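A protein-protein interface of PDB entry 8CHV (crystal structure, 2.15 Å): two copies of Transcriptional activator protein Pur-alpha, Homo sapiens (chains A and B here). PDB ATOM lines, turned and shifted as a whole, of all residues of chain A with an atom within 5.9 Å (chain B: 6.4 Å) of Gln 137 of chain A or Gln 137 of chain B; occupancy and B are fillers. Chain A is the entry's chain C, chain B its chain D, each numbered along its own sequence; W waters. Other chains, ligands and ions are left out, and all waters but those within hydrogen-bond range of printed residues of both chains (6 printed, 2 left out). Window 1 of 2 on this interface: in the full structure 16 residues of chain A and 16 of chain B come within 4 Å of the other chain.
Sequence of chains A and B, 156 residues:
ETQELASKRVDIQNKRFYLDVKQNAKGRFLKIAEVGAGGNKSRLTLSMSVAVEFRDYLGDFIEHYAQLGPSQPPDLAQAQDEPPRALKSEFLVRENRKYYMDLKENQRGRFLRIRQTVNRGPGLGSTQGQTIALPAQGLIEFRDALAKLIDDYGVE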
ATOM      1  N   ASP A  11      -1.294   0.637  -9.445  1.00  0.00           N
ATOM      2  CA  ASP A  11      -1.833   1.437  -8.358  1.00  0.00           C
ATOM      3  C   ASP A  11      -3.334   1.584  -8.549  1.00  0.00           C
ATOM      4  O   ASP A  11      -3.766   1.928  -9.637  1.00  0.00           O
ATOM      5  CB  ASP A  11      -1.140   2.795  -8.301  1.00  0.00           C
ATOM      6  CG  ASP A  11       0.353   2.651  -8.098  1.00  0.00           C
ATOM      7  OD1 ASP A  11       0.756   2.353  -6.966  1.00  0.00           O
ATOM      8  OD2 ASP A  11       1.094   2.806  -9.074  1.00  0.00           O
ATOM      9  N   ILE A  12      -4.114   1.304  -7.498  1.00  0.00           N
ATOM     10  CA  ILE A  12      -5.567   1.377  -7.571  1.00  0.00           C
ATOM     11  C   ILE A  12      -6.073   1.987  -6.272  1.00  0.00           C
ATOM     12  O   ILE A  12      -5.930   1.360  -5.221  1.00  0.00           O
ATOM     13  CB  ILE A  12      -6.223  -0.006  -7.789  1.00  0.00           C
ATOM     14  CG1 ILE A  12      -5.547  -0.837  -8.876  1.00  0.00           C
ATOM     15  CG2 ILE A  12      -7.710   0.154  -8.062  1.00  0.00           C
ATOM     16  CD1 ILE A  12      -5.997  -2.295  -8.903  1.00  0.00           C
ATOM     17  N   GLN A  13      -6.735   3.150  -6.379  1.00  0.00           N
ATOM     18  CA  GLN A  13      -7.061   3.995  -5.235  1.00  0.00           C
ATOM     19  C   GLN A  13      -5.788   4.089  -4.387  1.00  0.00           C
ATOM     20  O   GLN A  13      -4.752   4.483  -4.922  1.00  0.00           O
ATOM     21  CB  GLN A  13      -8.335   3.503  -4.531  1.00  0.00           C
ATOM     22  CG  GLN A  13      -9.599   3.479  -5.411  1.00  0.00           C
ATOM     23  CD  GLN A  13      -9.983   4.786  -6.093  1.00  0.00           C
ATOM     24  OE1 GLN A  13      -9.451   5.152  -7.140  1.00  0.00           O
ATOM     25  NE2 GLN A  13     -10.973   5.486  -5.561  1.00  0.00           N
ATOM     26  N   TYR A  65     -18.864  -5.605 -14.858  1.00  0.00           N
ATOM     27  CA  TYR A  65     -18.749  -4.334 -14.135  1.00  0.00           C
ATOM     28  C   TYR A  65     -19.137  -3.147 -15.018  1.00  0.00           C
ATOM     29  O   TYR A  65     -19.874  -2.282 -14.567  1.00  0.00           O
ATOM     30  CB  TYR A  65     -17.341  -4.204 -13.545  1.00  0.00           C
ATOM     31  CG  TYR A  65     -16.934  -2.866 -12.974  1.00  0.00           C
ATOM     32  CD1 TYR A  65     -17.702  -2.197 -12.036  1.00  0.00           C
ATOM     33  CD2 TYR A  65     -15.725  -2.285 -13.342  1.00  0.00           C
ATOM     34  CE1 TYR A  65     -17.290  -0.983 -11.501  1.00  0.00           C
ATOM     35  CE2 TYR A  65     -15.301  -1.074 -12.813  1.00  0.00           C
ATOM     36  CZ  TYR A  65     -16.091  -0.412 -11.899  1.00  0.00           C
ATOM     37  OH  TYR A  65     -15.648   0.780 -11.397  1.00  0.00           O
ATOM     38  N   ARG A 108     -18.154   1.131   0.416  1.00  0.00           N
ATOM     39  CA  ARG A 108     -17.159   1.996  -0.206  1.00  0.00           C
ATOM     40  C   ARG A 108     -17.095   1.768  -1.727  1.00  0.00           C
ATOM     41  O   ARG A 108     -16.624   2.641  -2.452  1.00  0.00           O
ATOM     42  CB  ARG A 108     -15.797   1.873   0.497  1.00  0.00           C
ATOM     43  CG  ARG A 108     -14.694   1.234  -0.339  1.00  0.00           C
ATOM     44  CD  ARG A 108     -13.278   1.572   0.111  1.00  0.00           C
ATOM     45  NE  ARG A 108     -12.802   0.691   1.174  1.00  0.00           N
ATOM     46  CZ  ARG A 108     -11.846  -0.232   1.039  1.00  0.00           C
ATOM     47  NH1 ARG A 108     -11.218  -0.390  -0.117  1.00  0.00           N
ATOM     48  NH2 ARG A 108     -11.525  -0.997   2.070  1.00  0.00           N
ATOM     49  N   ARG A 110     -17.376  -1.298  -5.394  1.00  0.00           N
ATOM     50  CA  ARG A 110     -17.273  -2.631  -5.966  1.00  0.00           C
ATOM     51  C   ARG A 110     -15.835  -3.141  -5.907  1.00  0.00           C
ATOM     52  O   ARG A 110     -14.894  -2.372  -5.988  1.00  0.00           O
ATOM     53  CB  ARG A 110     -17.697  -2.652  -7.438  1.00  0.00           C
ATOM     54  CG  ARG A 110     -19.197  -2.578  -7.696  1.00  0.00           C
ATOM     55  CD  ARG A 110     -19.753  -1.173  -7.894  1.00  0.00           C
ATOM     56  NE  ARG A 110     -20.992  -1.192  -8.673  1.00  0.00           N
ATOM     57  CZ  ARG A 110     -21.230  -0.435  -9.748  1.00  0.00           C
ATOM     58  NH1 ARG A 110     -20.382   0.520 -10.112  1.00  0.00           N
ATOM     59  NH2 ARG A 110     -22.354  -0.601 -10.429  1.00  0.00           N
ATOM     60  N   PRO A 135     -10.011  -3.232  -5.991  1.00  0.00           N
ATOM     61  CA  PRO A 135     -11.107  -2.322  -6.329  1.00  0.00           C
ATOM     62  C   PRO A 135     -11.408  -2.432  -7.819  1.00  0.00           C
ATOM     63  O   PRO A 135     -10.473  -2.578  -8.606  1.00  0.00           O
ATOM     64  CB  PRO A 135     -10.515  -0.959  -5.982  1.00  0.00           C
ATOM     65  CG  PRO A 135      -9.486  -1.278  -4.936  1.00  0.00           C
ATOM     66  CD  PRO A 135      -8.834  -2.529  -5.471  1.00  0.00           C
ATOM     67  N   ALA A 136     -12.702  -2.356  -8.182  1.00  0.00           N
ATOM     68  CA  ALA A 136     -13.175  -2.687  -9.522  1.00  0.00           C
ATOM     69  C   ALA A 136     -12.612  -1.719 -10.553  1.00  0.00           C
ATOM     70  O   ALA A 136     -12.292  -2.119 -11.666  1.00  0.00           O
ATOM     71  CB  ALA A 136     -14.690  -2.736  -9.570  1.00  0.00           C
ATOM     72  N   GLN A 137     -12.409  -0.472 -10.136  1.00  0.00           N
ATOM     73  CA  GLN A 137     -11.820   0.583 -10.956  1.00  0.00           C
ATOM     74  C   GLN A 137     -10.509   0.128 -11.580  1.00  0.00           C
ATOM     75  O   GLN A 137     -10.200   0.523 -12.700  1.00  0.00           O
ATOM     76  CB  GLN A 137     -11.565   1.838 -10.118  1.00  0.00           C
ATOM     77  CG  GLN A 137     -12.838   2.421  -9.532  1.00  0.00           C
ATOM     78  CD  GLN A 137     -13.087   1.981  -8.109  1.00  0.00           C
ATOM     79  OE1 GLN A 137     -13.061   0.786  -7.775  1.00  0.00           O
ATOM     80  NE2 GLN A 137     -13.313   2.968  -7.249  1.00  0.00           N
ATOM     81  N   GLY A 138      -9.742  -0.706 -10.869  1.00  0.00           N
ATOM     82  CA  GLY A 138      -8.422  -1.123 -11.336  1.00  0.00           C
ATOM     83  C   GLY A 138      -8.382  -2.476 -12.060  1.00  0.00           C
ATOM     84  O   GLY A 138      -7.299  -2.933 -12.404  1.00  0.00           O
ATOM     85  N   LEU A 139      -9.522  -3.125 -12.323  1.00  0.00           N
ATOM     86  CA  LEU A 139      -9.451  -4.453 -12.931  1.00  0.00           C
ATOM     87  C   LEU A 139      -8.786  -4.376 -14.298  1.00  0.00           C
ATOM     88  O   LEU A 139      -8.086  -5.308 -14.700  1.00  0.00           O
ATOM     89  CB  LEU A 139     -10.852  -5.070 -13.102  1.00  0.00           C
ATOM     90  CG  LEU A 139     -11.568  -5.432 -11.802  1.00  0.00           C
ATOM     91  CD1 LEU A 139     -12.963  -5.960 -12.093  1.00  0.00           C
ATOM     92  CD2 LEU A 139     -10.735  -6.427 -10.988  1.00  0.00           C
ATOM     93  N   ILE A 140      -9.091  -3.308 -15.041  1.00  0.00           N
ATOM     94  CA  ILE A 140      -8.617  -3.222 -16.404  1.00  0.00           C
ATOM     95  C   ILE A 140      -7.098  -3.065 -16.376  1.00  0.00           C
ATOM     96  O   ILE A 140      -6.403  -3.755 -17.118  1.00  0.00           O
ATOM     97  CB  ILE A 140      -9.356  -2.120 -17.194  1.00  0.00           C
ATOM     98  CG1 ILE A 140     -10.818  -2.495 -17.435  1.00  0.00           C
ATOM     99  CG2 ILE A 140      -8.664  -1.845 -18.527  1.00  0.00           C
ATOM    100  CD1 ILE A 140     -11.696  -1.366 -17.992  1.00  0.00           C
ATOM    101  N   GLU A 141      -6.580  -2.159 -15.535  1.00  0.00           N
ATOM    102  CA  GLU A 141      -5.138  -1.958 -15.455  1.00  0.00           C
ATOM    103  C   GLU A 141      -4.462  -3.244 -14.978  1.00  0.00           C
ATOM    104  O   GLU A 141      -3.394  -3.623 -15.440  1.00  0.00           O
ATOM    105  CB  GLU A 141      -4.779  -0.809 -14.504  1.00  0.00           C
ATOM    106  CG  GLU A 141      -5.264   0.541 -14.981  1.00  0.00           C
ATOM    107  CD  GLU A 141      -4.824   0.930 -16.383  1.00  0.00           C
ATOM    108  OE1 GLU A 141      -3.769   0.430 -16.824  1.00  0.00           O
ATOM    109  OE2 GLU A 141      -5.549   1.700 -17.052  1.00  0.00           O
ATOM    110  N   ASP B  11     -14.409   9.786  -6.375  1.00  0.00           N
ATOM    111  CA  ASP B  11     -12.969   9.860  -6.184  1.00  0.00           C
ATOM    112  C   ASP B  11     -12.324   8.872  -7.143  1.00  0.00           C
ATOM    113  O   ASP B  11     -12.696   7.703  -7.155  1.00  0.00           O
ATOM    114  CB  ASP B  11     -12.566   9.579  -4.735  1.00  0.00           C
ATOM    115  CG  ASP B  11     -13.057  10.649  -3.779  1.00  0.00           C
ATOM    116  OD1 ASP B  11     -12.665  11.818  -3.955  1.00  0.00           O
ATOM    117  OD2 ASP B  11     -13.866  10.314  -2.908  1.00  0.00           O
ATOM    118  N   ILE B  12     -11.390   9.367  -7.958  1.00  0.00           N
ATOM    119  CA  ILE B  12     -10.718   8.534  -8.929  1.00  0.00           C
ATOM    120  C   ILE B  12      -9.237   8.714  -8.696  1.00  0.00           C
ATOM    121  O   ILE B  12      -8.737   9.819  -8.903  1.00  0.00           O
ATOM    122  CB  ILE B  12     -11.083   8.906 -10.381  1.00  0.00           C
ATOM    123  CG1 ILE B  12     -12.587   8.771 -10.642  1.00  0.00           C
ATOM    124  CG2 ILE B  12     -10.250   8.070 -11.354  1.00  0.00           C
ATOM    125  CD1 ILE B  12     -13.034   9.202 -12.026  1.00  0.00           C
ATOM    126  N   GLN B  13      -8.569   7.590  -8.399  1.00  0.00           N
ATOM    127  CA  GLN B  13      -7.189   7.561  -7.955  1.00  0.00           C
ATOM    128  C   GLN B  13      -7.074   8.562  -6.813  1.00  0.00           C
ATOM    129  O   GLN B  13      -7.705   8.365  -5.769  1.00  0.00           O
ATOM    130  CB  GLN B  13      -6.191   7.812  -9.091  1.00  0.00           C
ATOM    131  CG  GLN B  13      -6.245   6.802 -10.228  1.00  0.00           C
ATOM    132  CD  GLN B  13      -5.590   5.486  -9.904  1.00  0.00           C
ATOM    133  OE1 GLN B  13      -4.700   5.036 -10.617  1.00  0.00           O
ATOM    134  NE2 GLN B  13      -6.046   4.842  -8.844  1.00  0.00           N
ATOM    135  N   TYR B  65     -11.631   1.577 -23.778  1.00  0.00           N
ATOM    136  CA  TYR B  65     -10.574   1.468 -22.773  1.00  0.00           C
ATOM    137  C   TYR B  65     -10.412   0.000 -22.366  1.00  0.00           C
ATOM    138  O   TYR B  65      -9.294  -0.510 -22.273  1.00  0.00           O
ATOM    139  CB  TYR B  65     -10.843   2.438 -21.608  1.00  0.00           C
ATOM    140  CG  TYR B  65     -10.046   2.208 -20.345  1.00  0.00           C
ATOM    141  CD1 TYR B  65      -8.670   2.170 -20.362  1.00  0.00           C
ATOM    142  CD2 TYR B  65     -10.675   2.055 -19.114  1.00  0.00           C
ATOM    143  CE1 TYR B  65      -7.935   1.955 -19.210  1.00  0.00           C
ATOM    144  CE2 TYR B  65      -9.959   1.846 -17.949  1.00  0.00           C
ATOM    145  CZ  TYR B  65      -8.585   1.803 -17.998  1.00  0.00           C
ATOM    146  OH  TYR B  65      -7.871   1.567 -16.861  1.00  0.00           O
ATOM    147  N   ARG B 110      -3.840   6.173 -18.676  1.00  0.00           N
ATOM    148  CA  ARG B 110      -4.914   6.541 -19.586  1.00  0.00           C
ATOM    149  C   ARG B 110      -5.935   7.472 -18.905  1.00  0.00           C
ATOM    150  O   ARG B 110      -6.288   7.256 -17.751  1.00  0.00           O
ATOM    151  CB  ARG B 110      -5.621   5.288 -20.120  1.00  0.00           C
ATOM    152  CG  ARG B 110      -4.793   4.409 -21.050  1.00  0.00           C
ATOM    153  CD  ARG B 110      -4.296   3.148 -20.376  1.00  0.00           C
ATOM    154  NE  ARG B 110      -3.800   2.150 -21.316  1.00  0.00           N
ATOM    155  CZ  ARG B 110      -4.082   0.843 -21.294  1.00  0.00           C
ATOM    156  NH1 ARG B 110      -4.689   0.270 -20.257  1.00  0.00           N
ATOM    157  NH2 ARG B 110      -3.681   0.108 -22.318  1.00  0.00           N
ATOM    158  N   LEU B 134     -10.315  12.932 -16.457  1.00  0.00           N
ATOM    159  CA  LEU B 134     -10.688  11.790 -15.645  1.00  0.00           C
ATOM    160  C   LEU B 134      -9.714  10.639 -15.870  1.00  0.00           C
ATOM    161  O   LEU B 134      -9.589  10.140 -16.994  1.00  0.00           O
ATOM    162  CB  LEU B 134     -12.081  11.332 -16.090  1.00  0.00           C
ATOM    163  CG  LEU B 134     -13.195  12.325 -15.828  1.00  0.00           C
ATOM    164  CD1 LEU B 134     -14.407  11.980 -16.661  1.00  0.00           C
ATOM    165  CD2 LEU B 134     -13.568  12.311 -14.359  1.00  0.00           C
ATOM    166  N   PRO B 135      -9.079  10.074 -14.829  1.00  0.00           N
ATOM    167  CA  PRO B 135      -8.287   8.866 -15.024  1.00  0.00           C
ATOM    168  C   PRO B 135      -9.193   7.745 -15.534  1.00  0.00           C
ATOM    169  O   PRO B 135     -10.303   7.569 -15.054  1.00  0.00           O
ATOM    170  CB  PRO B 135      -7.708   8.578 -13.639  1.00  0.00           C
ATOM    171  CG  PRO B 135      -7.803   9.884 -12.898  1.00  0.00           C
ATOM    172  CD  PRO B 135      -9.052  10.547 -13.444  1.00  0.00           C
ATOM    173  N   ALA B 136      -8.734   7.003 -16.541  1.00  0.00           N
ATOM    174  CA  ALA B 136      -9.606   6.066 -17.238  1.00  0.00           C
ATOM    175  C   ALA B 136     -10.119   4.981 -16.300  1.00  0.00           C
ATOM    176  O   ALA B 136     -11.207   4.475 -16.515  1.00  0.00           O
ATOM    177  CB  ALA B 136      -8.900   5.454 -18.400  1.00  0.00           C
ATOM    178  N   GLN B 137      -9.368   4.663 -15.241  1.00  0.00           N
ATOM    179  CA  GLN B 137      -9.798   3.632 -14.315  1.00  0.00           C
ATOM    180  C   GLN B 137     -11.057   4.076 -13.565  1.00  0.00           C
ATOM    181  O   GLN B 137     -11.730   3.222 -12.991  1.00  0.00           O
ATOM    182  CB  GLN B 137      -8.655   3.206 -13.385  1.00  0.00           C
ATOM    183  CG  GLN B 137      -8.527   4.015 -12.102  1.00  0.00           C
ATOM    184  CD  GLN B 137      -7.676   3.260 -11.107  1.00  0.00           C
ATOM    185  OE1 GLN B 137      -8.025   3.111  -9.938  1.00  0.00           O
ATOM    186  NE2 GLN B 137      -6.553   2.745 -11.582  1.00  0.00           N
ATOM    187  N   GLY B 138     -11.410   5.376 -13.619  1.00  0.00           N
ATOM    188  CA  GLY B 138     -12.610   5.880 -12.959  1.00  0.00           C
ATOM    189  C   GLY B 138     -13.832   6.097 -13.856  1.00  0.00           C
ATOM    190  O   GLY B 138     -14.856   6.540 -13.356  1.00  0.00           O
ATOM    191  N   LEU B 139     -13.756   5.812 -15.166  1.00  0.00           N
ATOM    192  CA  LEU B 139     -14.844   6.160 -16.085  1.00  0.00           C
ATOM    193  C   LEU B 139     -16.142   5.430 -15.755  1.00  0.00           C
ATOM    194  O   LEU B 139     -17.228   5.999 -15.953  1.00  0.00           O
ATOM    195  CB  LEU B 139     -14.453   5.823 -17.526  1.00  0.00           C
ATOM    196  CG  LEU B 139     -13.243   6.593 -18.028  1.00  0.00           C
ATOM    197  CD1 LEU B 139     -12.758   6.058 -19.368  1.00  0.00           C
ATOM    198  CD2 LEU B 139     -13.586   8.053 -18.119  1.00  0.00           C
ATOM    199  N   ILE B 140     -16.025   4.159 -15.336  1.00  0.00           N
ATOM    200  CA  ILE B 140     -17.223   3.398 -15.058  1.00  0.00           C
ATOM    201  C   ILE B 140     -17.947   4.010 -13.855  1.00  0.00           C
ATOM    202  O   ILE B 140     -19.174   4.203 -13.904  1.00  0.00           O
ATOM    203  CB  ILE B 140     -16.911   1.904 -14.906  1.00  0.00           C
ATOM    204  CG1 ILE B 140     -16.591   1.290 -16.269  1.00  0.00           C
ATOM    205  CG2 ILE B 140     -18.054   1.187 -14.208  1.00  0.00           C
ATOM    206  CD1 ILE B 140     -15.844  -0.008 -16.198  1.00  0.00           C
ATOM    207  N   GLU B 141     -17.194   4.355 -12.801  1.00  0.00           N
ATOM    208  CA  GLU B 141     -17.781   5.024 -11.646  1.00  0.00           C
ATOM    209  C   GLU B 141     -18.432   6.344 -12.074  1.00  0.00           C
ATOM    210  O   GLU B 141     -19.592   6.610 -11.793  1.00  0.00           O
ATOM    211  CB  GLU B 141     -16.743   5.274 -10.548  1.00  0.00           C
ATOM    212  CG  GLU B 141     -16.336   4.036  -9.763  1.00  0.00           C
ATOM    213  CD  GLU B 141     -17.426   3.089  -9.279  1.00  0.00           C
ATOM    214  OE1 GLU B 141     -18.288   3.549  -8.515  1.00  0.00           O
ATOM    215  OE2 GLU B 141     -17.403   1.885  -9.660  1.00  0.00           O
HETATM  216  O   HOH W   1     -13.836   5.780  -8.613  1.00  0.00           O
HETATM  217  O   HOH W   2     -14.556   2.924 -12.848  1.00  0.00           O
HETATM  218  O   HOH W   3      -8.439  -0.237 -14.570  1.00  0.00           O
HETATM  219  O   HOH W   4      -4.578   4.312 -16.628  1.00  0.00           O
HETATM  220  O   HOH W   5     -12.439   0.906 -14.802  1.00  0.00           O
HETATM  221  O   HOH W   6      -3.731   4.516  -7.155  1.00  0.00           O
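The backbone carbonyl oxygen (O) of Arg 110 of chain A is in hydrogen-bond range of the backbone NH (N) of Ala 136 of chain A (3.1 Å).
NE2 of Gln 13 of chain B is in hydrogen-bond range of OE1 of Gln 137 of chain B (2.8 Å).
The backbone carbonyl oxygen of Arg 110 of chain B lies within hydrogen-bond range of the backbone NH of Ala 136 of chain B (2.7 Å).
Among the printed residues, pairs that only touch across the chains: Ile 12 of chain A with Gln 13 of chain B, Ile 12 of chain A with Gln 137 of chain B, Gln 13 of chain A with Ile 12 of chain B, Gln 13 of chain A with Gln 137 of chain B, Tyr 65 of chain A with Ile 140 of chain B, Gln 137 of chain A with Glu 141 of chain B and Ile 140 of chain A with Tyr 65 of chain B.
The side-chain carboxylate (OE1) of Glu 141 of chain A lies within salt-bridge range of the guanidinium group (NH1) of Arg 110 of chain B, at 3.6 Å.
The side-chain amide nitrogen (NE2) of Gln 137 of chain B is in hydrogen-bond range of the backbone carbonyl oxygen (O) of Asp 11 of chain A (3.5 Å).
O of Asp 11 of chain B sits at hydrogen-bond distance from NE2 of Gln 13 of chain A, 3.2 Å away.
OE1 of Gln 13 of chain A lies within hydrogen-bond range of N of Gln 13 of chain B.
The guanidinium group of Arg 110 of chain A is in salt-bridge range of the side-chain carboxylate of Glu 141 of chain B, 3.3 Å away.
The side-chain amide oxygen (OE1) of Gln 13 of chain B lies close to the backbone carbonyl oxygen (O) of Asp 11 of chain A, at 3.4 Å.
The side-chain carboxylate of Glu 141 of chain B sits at hydrogen-bond distance from the side-chain hydroxyl of Tyr 65 of chain A (2.7 Å).
The side-chain carboxylate (OE2) of Glu 141 of chain A lies close to the side-chain hydroxyl (OH) of Tyr 65 of chain B, 2.3 Å away.
The backbone carbonyl oxygen of Gln 137 of chain A sits close to the backbone carbonyl oxygen of Gln 137 of chain B.
Pro 135 of chain A touches none of the printed residues of chain B.
Of the printed residues of chain B, Gln 137 of chain A touches Gln 137 and Glu 141.
Printed residues of chain B within 4 Å of Ile 140 of chain A: Tyr 65 (3.7 Å).
Printed residues of chain A within 4 Å of Asp 11 of chain B: Gln 13 (3.2 Å).
Of the printed residues of chain A, Gln 137 of chain B touches Asp 11 (3.5 Å), Ile 12 (3.5 Å), Gln 13 (3.7 Å) and Gln 137 (3.1 Å).
Printed residues of chain A within 4 Å of Ile 140 of chain B: Tyr 65 (3.4 Å).
The nearest printed residue of chain B that does not touch Gln 137 of chain A is Asp 11 of chain B (4.8 Å).
The nearest printed residue of chain A that does not touch Gln 137 of chain B is Glu 141 of chain A (4.3 Å).
The nearest printed residue of chain B that does not touch Tyr 65 of chain A is Gln 137 of chain B (4.9 Å).
Asp 11 of chain A touches Gln 137 of chain B, but with the chains exchanged Gln 137 of chain A does not touch Asp 11 of chain B (4.8 Å).
Gln 13 of chain A touches its own counterpart, Gln 13 of chain B.
Gln 13 of chain A touches Gln 137 of chain B, but with the chains exchanged Gln 137 of chain A does not touch Gln 13 of chain B (6.4 Å).
Gln 137 of chain A touches Glu 141 of chain B, but with the chains exchanged Glu 141 of chain A does not touch Gln 137 of chain B (4.3 Å).
Of the 16 pairs that touch across the chains among the printed residues, 12 have their exchanged pair printed and touching as well.
Water W6 lies within hydrogen-bond range of the backbone carbonyl oxygen of Gln 13 of chain A (2.5 Å), the side-chain amide nitrogen of Gln 13 of chain B (2.9 Å) and the backbone NH of Ile 12 of chain A (3.3 Å).
Water W1 bridges O of Asp 11 of chain B (2.7 Å) and NE2 of Gln 137 of chain A (3.2 Å).
Water W3 lies within hydrogen-bond range of the backbone carbonyl oxygen of Gln 137 of chain A (2.7 Å), the backbone NH of Glu 141 of chain A (2.8 Å), the side-chain hydroxyl of Tyr 65 of chain B (3.0 Å) and the backbone NH of Ile 140 of chain A (3.2 Å).
Water W2 lies within hydrogen-bond range of OH of Tyr 65 of chain A (2.8 Å), O of Gln 137 of chain B (2.8 Å), N of Glu 141 of chain B (3.0 Å) and N of Ile 140 of chain B (3.1 Å).
Water W4 lies within hydrogen-bond range of OE2 of Glu 141 of chain A and N of Arg 110 of chain B.
Water W5 lies within hydrogen-bond range of the backbone carbonyl oxygen (O) of Gln 137 of chain B (3.0 Å) and the backbone carbonyl oxygen (O) of Gln 137 of chain A (3.1 Å).
Of the 13 printed residues of chain B, 8 touch a printed residue of chain A.
Printed residues of chain B that touch a printed residue of chain A: Asp 11, Ile 12, Gln 13, Tyr 65, Arg 110, Gln 137, Ile 140 and Glu 141.
Hydrophobic or aromatic side chains of chain B that line the printed part of chain A: Tyr 65 and Ile 140.
Printed residues of chain A that touch a printed residue of chain B: Asp 11, Ile 12, Gln 13, Tyr 65, Arg 110, Gln 137, Ile 140 and Glu 141.
Hydrophobic or aromatic side chains of chain A within 4 Å of the printed part of chain B: Ile 12, Tyr 65 and Ile 140.
Among the printed residues, Asp or Glu carboxylates within 4 Å of a Lys or Arg side-chain nitrogen of the other chain: Arg 110 of chain A with Glu 141 of chain B and Glu 141 of chain A with Arg 110 of chain B.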
